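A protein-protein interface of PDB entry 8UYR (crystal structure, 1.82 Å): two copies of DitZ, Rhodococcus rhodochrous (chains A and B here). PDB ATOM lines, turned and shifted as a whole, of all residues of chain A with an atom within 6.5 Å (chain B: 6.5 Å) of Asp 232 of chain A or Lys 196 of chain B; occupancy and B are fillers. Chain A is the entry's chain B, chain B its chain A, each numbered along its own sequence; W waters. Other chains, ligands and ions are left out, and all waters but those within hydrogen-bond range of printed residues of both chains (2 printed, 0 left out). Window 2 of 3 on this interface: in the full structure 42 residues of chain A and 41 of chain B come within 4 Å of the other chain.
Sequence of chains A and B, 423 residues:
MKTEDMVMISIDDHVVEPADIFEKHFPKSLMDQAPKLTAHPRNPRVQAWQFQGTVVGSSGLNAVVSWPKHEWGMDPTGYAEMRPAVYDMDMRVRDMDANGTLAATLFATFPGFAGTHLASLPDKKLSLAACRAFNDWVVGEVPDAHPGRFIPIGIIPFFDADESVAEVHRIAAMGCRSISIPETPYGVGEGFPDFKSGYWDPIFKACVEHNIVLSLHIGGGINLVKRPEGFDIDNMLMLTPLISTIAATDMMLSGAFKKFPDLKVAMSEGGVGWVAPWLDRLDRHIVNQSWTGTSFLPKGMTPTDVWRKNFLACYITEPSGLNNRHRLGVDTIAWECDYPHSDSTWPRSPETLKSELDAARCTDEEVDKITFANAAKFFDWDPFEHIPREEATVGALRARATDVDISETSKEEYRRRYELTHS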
ATOM      1  N   GLY A 230     -12.950   2.617  -6.234  1.00  0.00           N
ATOM      2  CA  GLY A 230     -13.919   3.130  -5.291  1.00  0.00           C
ATOM      3  C   GLY A 230     -14.558   2.061  -4.412  1.00  0.00           C
ATOM      4  O   GLY A 230     -15.450   1.361  -4.777  1.00  0.00           O
ATOM      5  N   PHE A 231     -14.065   1.983  -3.210  1.00  0.00           N
ATOM      6  CA  PHE A 231     -14.482   1.037  -2.182  1.00  0.00           C
ATOM      7  C   PHE A 231     -15.927   1.143  -1.671  1.00  0.00           C
ATOM      8  O   PHE A 231     -16.403   2.225  -1.388  1.00  0.00           O
ATOM      9  CB  PHE A 231     -13.463   1.278  -1.081  1.00  0.00           C
ATOM     10  CG  PHE A 231     -13.747   0.618   0.202  1.00  0.00           C
ATOM     11  CD1 PHE A 231     -13.029  -0.485   0.574  1.00  0.00           C
ATOM     12  CD2 PHE A 231     -14.641   1.165   1.085  1.00  0.00           C
ATOM     13  CE1 PHE A 231     -13.238  -1.074   1.796  1.00  0.00           C
ATOM     14  CE2 PHE A 231     -14.870   0.591   2.295  1.00  0.00           C
ATOM     15  CZ  PHE A 231     -14.171  -0.547   2.653  1.00  0.00           C
ATOM     16  N   ASP A 232     -16.625   0.017  -1.602  1.00  0.00           N
ATOM     17  CA  ASP A 232     -17.959  -0.014  -1.061  1.00  0.00           C
ATOM     18  C   ASP A 232     -17.936  -1.115  -0.038  1.00  0.00           C
ATOM     19  O   ASP A 232     -17.875  -2.267  -0.407  1.00  0.00           O
ATOM     20  CB  ASP A 232     -19.011  -0.325  -2.110  1.00  0.00           C
ATOM     21  CG  ASP A 232     -20.432  -0.161  -1.602  1.00  0.00           C
ATOM     22  OD1 ASP A 232     -21.374  -0.303  -2.395  1.00  0.00           O
ATOM     23  OD2 ASP A 232     -20.623   0.104  -0.408  1.00  0.00           O
ATOM     24  N   ILE A 233     -17.937  -0.741   1.226  1.00  0.00           N
ATOM     25  CA  ILE A 233     -17.982  -1.657   2.324  1.00  0.00           C
ATOM     26  C   ILE A 233     -19.109  -2.659   2.103  1.00  0.00           C
ATOM     27  O   ILE A 233     -18.904  -3.838   2.195  1.00  0.00           O
ATOM     28  CB  ILE A 233     -18.168  -0.878   3.644  1.00  0.00           C
ATOM     29  CG1 ILE A 233     -18.439  -1.785   4.816  1.00  0.00           C
ATOM     30  CG2 ILE A 233     -19.347   0.044   3.591  1.00  0.00           C
ATOM     31  CD1 ILE A 233     -18.731  -0.983   6.058  1.00  0.00           C
ATOM     32  N   ASP A 234     -20.278  -2.156   1.784  1.00  0.00           N
ATOM     33  CA  ASP A 234     -21.382  -3.010   1.507  1.00  0.00           C
ATOM     34  C   ASP A 234     -21.037  -4.004   0.410  1.00  0.00           C
ATOM     35  O   ASP A 234     -21.475  -5.082   0.483  1.00  0.00           O
ATOM     36  CB  ASP A 234     -22.578  -2.178   1.076  1.00  0.00           C
ATOM     37  CG  ASP A 234     -23.329  -1.572   2.238  1.00  0.00           C
ATOM     38  OD1 ASP A 234     -24.342  -0.950   1.992  1.00  0.00           O
ATOM     39  OD2 ASP A 234     -22.928  -1.743   3.364  1.00  0.00           O
ATOM     40  N   ASN A 235     -20.348  -3.607  -0.644  1.00  0.00           N
ATOM     41  CA  ASN A 235     -20.034  -4.558  -1.707  1.00  0.00           C
ATOM     42  C   ASN A 235     -19.135  -5.669  -1.181  1.00  0.00           C
ATOM     43  O   ASN A 235     -19.377  -6.860  -1.425  1.00  0.00           O
ATOM     44  CB  ASN A 235     -19.381  -3.823  -2.879  1.00  0.00           C
ATOM     45  CG  ASN A 235     -19.303  -4.667  -4.141  1.00  0.00           C
ATOM     46  OD1 ASN A 235     -18.709  -5.749  -4.147  1.00  0.00           O
ATOM     47  ND2 ASN A 235     -19.894  -4.166  -5.223  1.00  0.00           N
ATOM     48  N   MET A 236     -18.099  -5.293  -0.432  1.00  0.00           N
ATOM     49  CA  MET A 236     -17.242  -6.289   0.202  1.00  0.00           C
ATOM     50  C   MET A 236     -18.048  -7.189   1.132  1.00  0.00           C
ATOM     51  O   MET A 236     -17.977  -8.421   1.035  1.00  0.00           O
ATOM     52  CB  MET A 236     -16.110  -5.590   0.959  1.00  0.00           C
ATOM     53  CG  MET A 236     -15.352  -6.468   1.941  1.00  0.00           C
ATOM     54  SD  MET A 236     -14.390  -5.479   3.115  1.00  0.00           S
ATOM     55  CE  MET A 236     -12.743  -6.149   2.857  1.00  0.00           C
ATOM     56  N   LEU A 237     -18.838  -6.587   2.030  1.00  0.00           N
ATOM     57  CA  LEU A 237     -19.615  -7.375   2.984  1.00  0.00           C
ATOM     58  C   LEU A 237     -20.609  -8.292   2.289  1.00  0.00           C
ATOM     59  O   LEU A 237     -21.011  -9.316   2.857  1.00  0.00           O
ATOM     60  CB  LEU A 237     -20.364  -6.460   3.957  1.00  0.00           C
ATOM     61  CG  LEU A 237     -19.522  -5.526   4.827  1.00  0.00           C
ATOM     62  CD1 LEU A 237     -20.363  -4.963   5.958  1.00  0.00           C
ATOM     63  CD2 LEU A 237     -18.271  -6.239   5.355  1.00  0.00           C
ATOM     64  N   PRO B 193     -14.817   2.754 -16.202  1.00  0.00           N
ATOM     65  CA  PRO B 193     -15.582   3.149 -15.014  1.00  0.00           C
ATOM     66  C   PRO B 193     -16.609   2.089 -14.635  1.00  0.00           C
ATOM     67  O   PRO B 193     -17.134   1.368 -15.490  1.00  0.00           O
ATOM     68  CB  PRO B 193     -16.257   4.461 -15.443  1.00  0.00           C
ATOM     69  CG  PRO B 193     -15.366   4.990 -16.529  1.00  0.00           C
ATOM     70  CD  PRO B 193     -14.887   3.771 -17.266  1.00  0.00           C
ATOM     71  N   ASP B 194     -16.892   1.995 -13.333  1.00  0.00           N
ATOM     72  CA  ASP B 194     -17.809   0.975 -12.840  1.00  0.00           C
ATOM     73  C   ASP B 194     -19.243   1.516 -12.821  1.00  0.00           C
ATOM     74  O   ASP B 194     -19.499   2.689 -13.095  1.00  0.00           O
ATOM     75  CB  ASP B 194     -17.382   0.466 -11.455  1.00  0.00           C
ATOM     76  CG  ASP B 194     -17.637   1.471 -10.329  1.00  0.00           C
ATOM     77  OD1 ASP B 194     -17.777   2.679 -10.584  1.00  0.00           O
ATOM     78  OD2 ASP B 194     -17.701   1.037  -9.161  1.00  0.00           O
ATOM     79  N   PHE B 195     -20.195   0.630 -12.521  1.00  0.00           N
ATOM     80  CA  PHE B 195     -21.600   1.015 -12.639  1.00  0.00           C
ATOM     81  C   PHE B 195     -21.991   2.044 -11.589  1.00  0.00           C
ATOM     82  O   PHE B 195     -22.943   2.809 -11.797  1.00  0.00           O
ATOM     83  CB  PHE B 195     -22.506  -0.217 -12.529  1.00  0.00           C
ATOM     84  CG  PHE B 195     -22.341  -1.197 -13.671  1.00  0.00           C
ATOM     85  CD1 PHE B 195     -22.198  -0.743 -14.973  1.00  0.00           C
ATOM     86  CD2 PHE B 195     -22.340  -2.569 -13.440  1.00  0.00           C
ATOM     87  CE1 PHE B 195     -22.034  -1.636 -16.026  1.00  0.00           C
ATOM     88  CE2 PHE B 195     -22.186  -3.464 -14.487  1.00  0.00           C
ATOM     89  CZ  PHE B 195     -22.030  -2.988 -15.784  1.00  0.00           C
ATOM     90  N   LYS B 196     -21.291   2.061 -10.461  1.00  0.00           N
ATOM     91  CA  LYS B 196     -21.609   2.984  -9.383  1.00  0.00           C
ATOM     92  C   LYS B 196     -21.100   4.388  -9.656  1.00  0.00           C
ATOM     93  O   LYS B 196     -21.527   5.324  -8.974  1.00  0.00           O
ATOM     94  CB  LYS B 196     -21.012   2.479  -8.067  1.00  0.00           C
ATOM     95  CG  LYS B 196     -21.646   3.103  -6.836  1.00  0.00           C
ATOM     96  CD  LYS B 196     -21.083   2.521  -5.547  1.00  0.00           C
ATOM     97  CE  LYS B 196     -21.768   3.164  -4.340  1.00  0.00           C
ATOM     98  NZ  LYS B 196     -21.231   2.674  -3.038  1.00  0.00           N
ATOM     99  N   SER B 197     -20.211   4.555 -10.638  1.00  0.00           N
ATOM    100  CA  SER B 197     -19.568   5.843 -10.870  1.00  0.00           C
ATOM    101  C   SER B 197     -20.500   6.866 -11.494  1.00  0.00           C
ATOM    102  O   SER B 197     -20.203   8.061 -11.438  1.00  0.00           O
ATOM    103  CB  SER B 197     -18.349   5.673 -11.776  1.00  0.00           C
ATOM    104  OG  SER B 197     -18.734   5.343 -13.111  1.00  0.00           O
ATOM    105  N   GLY B 198     -21.616   6.434 -12.082  1.00  0.00           N
ATOM    106  CA  GLY B 198     -22.457   7.321 -12.849  1.00  0.00           C
ATOM    107  C   GLY B 198     -22.100   7.403 -14.315  1.00  0.00           C
ATOM    108  O   GLY B 198     -22.880   7.958 -15.098  1.00  0.00           O
ATOM    109  N   TYR B 199     -20.943   6.863 -14.708  1.00  0.00           N
ATOM    110  CA  TYR B 199     -20.511   6.928 -16.099  1.00  0.00           C
ATOM    111  C   TYR B 199     -21.544   6.316 -17.037  1.00  0.00           C
ATOM    112  O   TYR B 199     -21.756   6.811 -18.155  1.00  0.00           O
ATOM    113  CB  TYR B 199     -19.169   6.219 -16.233  1.00  0.00           C
ATOM    114  CG  TYR B 199     -18.658   6.061 -17.639  1.00  0.00           C
ATOM    115  CD1 TYR B 199     -17.903   7.060 -18.242  1.00  0.00           C
ATOM    116  CD2 TYR B 199     -18.902   4.893 -18.362  1.00  0.00           C
ATOM    117  CE1 TYR B 199     -17.412   6.908 -19.539  1.00  0.00           C
ATOM    118  CE2 TYR B 199     -18.425   4.737 -19.656  1.00  0.00           C
ATOM    119  CZ  TYR B 199     -17.684   5.744 -20.239  1.00  0.00           C
ATOM    120  OH  TYR B 199     -17.206   5.592 -21.516  1.00  0.00           O
ATOM    121  N   TRP B 200     -22.201   5.249 -16.596  1.00  0.00           N
ATOM    122  CA  TRP B 200     -23.116   4.511 -17.452  1.00  0.00           C
ATOM    123  C   TRP B 200     -24.526   5.078 -17.427  1.00  0.00           C
ATOM    124  O   TRP B 200     -25.377   4.628 -18.211  1.00  0.00           O
ATOM    125  CB  TRP B 200     -23.136   3.035 -17.035  1.00  0.00           C
ATOM    126  CG  TRP B 200     -21.796   2.384 -17.171  1.00  0.00           C
ATOM    127  CD1 TRP B 200     -20.765   2.440 -16.281  1.00  0.00           C
ATOM    128  CD2 TRP B 200     -21.348   1.560 -18.257  1.00  0.00           C
ATOM    129  NE1 TRP B 200     -19.696   1.720 -16.750  1.00  0.00           N
ATOM    130  CE2 TRP B 200     -20.024   1.169 -17.962  1.00  0.00           C
ATOM    131  CE3 TRP B 200     -21.932   1.127 -19.449  1.00  0.00           C
ATOM    132  CZ2 TRP B 200     -19.269   0.370 -18.818  1.00  0.00           C
ATOM    133  CZ3 TRP B 200     -21.176   0.315 -20.308  1.00  0.00           C
ATOM    134  CH2 TRP B 200     -19.863  -0.056 -19.981  1.00  0.00           C
ATOM    135  N   ASP B 201     -24.787   6.056 -16.556  1.00  0.00           N
ATOM    136  CA  ASP B 201     -26.158   6.522 -16.368  1.00  0.00           C
ATOM    137  C   ASP B 201     -26.821   6.998 -17.659  1.00  0.00           C
ATOM    138  O   ASP B 201     -28.008   6.693 -17.854  1.00  0.00           O
ATOM    139  CB  ASP B 201     -26.180   7.618 -15.295  1.00  0.00           C
ATOM    140  CG  ASP B 201     -25.976   7.064 -13.895  1.00  0.00           C
ATOM    141  OD1 ASP B 201     -25.757   5.843 -13.768  1.00  0.00           O
ATOM    142  OD2 ASP B 201     -26.047   7.845 -12.925  1.00  0.00           O
ATOM    143  N   ASP B 250     -22.518  -5.878  -8.003  1.00  0.00           N
ATOM    144  CA  ASP B 250     -22.148  -4.536  -8.465  1.00  0.00           C
ATOM    145  C   ASP B 250     -23.365  -3.759  -8.967  1.00  0.00           C
ATOM    146  O   ASP B 250     -23.554  -2.589  -8.621  1.00  0.00           O
ATOM    147  CB  ASP B 250     -21.106  -4.595  -9.584  1.00  0.00           C
ATOM    148  CG  ASP B 250     -19.788  -5.229  -9.152  1.00  0.00           C
ATOM    149  OD1 ASP B 250     -19.482  -5.239  -7.936  1.00  0.00           O
ATOM    150  OD2 ASP B 250     -19.054  -5.707 -10.048  1.00  0.00           O
ATOM    151  N   LEU B 253     -25.876  -2.889  -6.028  1.00  0.00           N
ATOM    152  CA  LEU B 253     -25.371  -1.915  -5.067  1.00  0.00           C
ATOM    153  C   LEU B 253     -24.993  -0.583  -5.701  1.00  0.00           C
ATOM    154  O   LEU B 253     -24.658   0.357  -4.974  1.00  0.00           O
ATOM    155  CB  LEU B 253     -24.139  -2.449  -4.339  1.00  0.00           C
ATOM    156  CG  LEU B 253     -24.267  -3.689  -3.432  1.00  0.00           C
ATOM    157  CD1 LEU B 253     -23.272  -3.659  -2.283  1.00  0.00           C
ATOM    158  CD2 LEU B 253     -25.679  -4.023  -2.970  1.00  0.00           C
ATOM    159  N   SER B 254     -25.010  -0.488  -7.029  1.00  0.00           N
ATOM    160  CA  SER B 254     -24.637   0.748  -7.705  1.00  0.00           C
ATOM    161  C   SER B 254     -25.665   1.842  -7.503  1.00  0.00           C
ATOM    162  O   SER B 254     -25.357   3.020  -7.741  1.00  0.00           O
ATOM    163  CB  SER B 254     -24.479   0.501  -9.207  1.00  0.00           C
ATOM    164  OG  SER B 254     -25.752   0.240  -9.785  1.00  0.00           O
ATOM    165  N   GLY B 255     -26.881   1.475  -7.092  1.00  0.00           N
ATOM    166  CA  GLY B 255     -27.992   2.397  -7.057  1.00  0.00           C
ATOM    167  C   GLY B 255     -28.662   2.586  -8.398  1.00  0.00           C
ATOM    168  O   GLY B 255     -29.529   3.454  -8.519  1.00  0.00           O
ATOM    169  N   LYS B 259     -32.121   4.940  -9.348  1.00  0.00           N
ATOM    170  CA  LYS B 259     -32.149   6.004 -10.347  1.00  0.00           C
ATOM    171  C   LYS B 259     -32.997   5.629 -11.556  1.00  0.00           C
ATOM    172  O   LYS B 259     -33.650   6.500 -12.135  1.00  0.00           O
ATOM    173  CB  LYS B 259     -30.733   6.358 -10.824  1.00  0.00           C
ATOM    174  CG  LYS B 259     -29.697   6.705  -9.741  1.00  0.00           C
ATOM    175  CD  LYS B 259     -28.333   7.123 -10.359  1.00  0.00           C
ATOM    176  CE  LYS B 259     -27.147   6.345  -9.743  1.00  0.00           C
ATOM    177  NZ  LYS B 259     -25.801   6.576 -10.409  1.00  0.00           N
HETATM  178  O   HOH W   1     -17.537   1.416  -6.574  1.00  0.00           O
HETATM  179  O   HOH W   2     -24.201   0.534  -2.034  1.00  0.00           O
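The side-chain amino group (NZ) of Lys 196 of chain B is in salt-bridge range of the side-chain carboxylate (OD1) of Asp 232 of chain A (3.0 Å).
OD1 of Asp 250 of chain B lies within hydrogen-bond range of ND2 of Asn 235 of chain A.
OD2 of Asp 232 of chain A sits close to N of Asp 234 of chain A (3.2 Å).
Leu 253 of chain B touches Asp 232 of chain A.
Asp 234 of chain A touches Leu 253 of chain B (C to CD1, 3.5 Å).
Leu 253 of chain B touches Asn 235 of chain A (CD1 to N, 3.4 Å).
Asp 232 of chain A touches just these residues of chain B: Lys 196 and Leu 253.
Of the printed residues of chain B, Asp 234 of chain A touches Leu 253 (3.5 Å).
Of the printed residues of chain B, Asn 235 of chain A touches Asp 250 and Leu 253.
Lys 196 of chain B touches just one residue of chain A: Asp 232 (3.0 Å).
Printed residues of chain A within 4 Å of Asp 250 of chain B: Asn 235 (2.9 Å).
Of the printed residues of chain A, Leu 253 of chain B touches Asp 232, Asp 234 and Asn 235.
The nearest residue of chain A that does not touch Lys 196 of chain B is Phe 231 of chain A (5.1 Å).
The nearest printed residue of chain B that does not touch Asn 235 of chain A is Ser 254 of chain B (6.6 Å).
Printed residues of chain B that touch a printed residue of chain A: Lys 196, Asp 250 and Leu 253.
Hydrophobic or aromatic side chains of chain B that line the printed part of chain A: Leu 253.
Along chain B the printed residues that touch a printed residue of chain A span positions 196 to 253.
Among the printed residues, 5 pairs touch across the chains.
Among the printed residues, Asp or Glu carboxylates within 4 Å of a Lys or Arg side-chain nitrogen of the other chain: Asp 232 of chain A with Lys 196 of chain B (3.0 Å).
No position is printed for both chains.
Of the 5 pairs that touch across the chains among the printed residues, none has its exchanged pair printed and touching as well.
Water W1 bridges OD2 of Asp 194 of chain B (2.6 Å) and O of Gly 230 of chain A (2.8 Å).
Water W2 lies within hydrogen-bond range of the side-chain carboxylate of Asp 232 of chain A (3.0 Å) and the backbone carbonyl oxygen of Leu 253 of chain B (3.0 Å).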
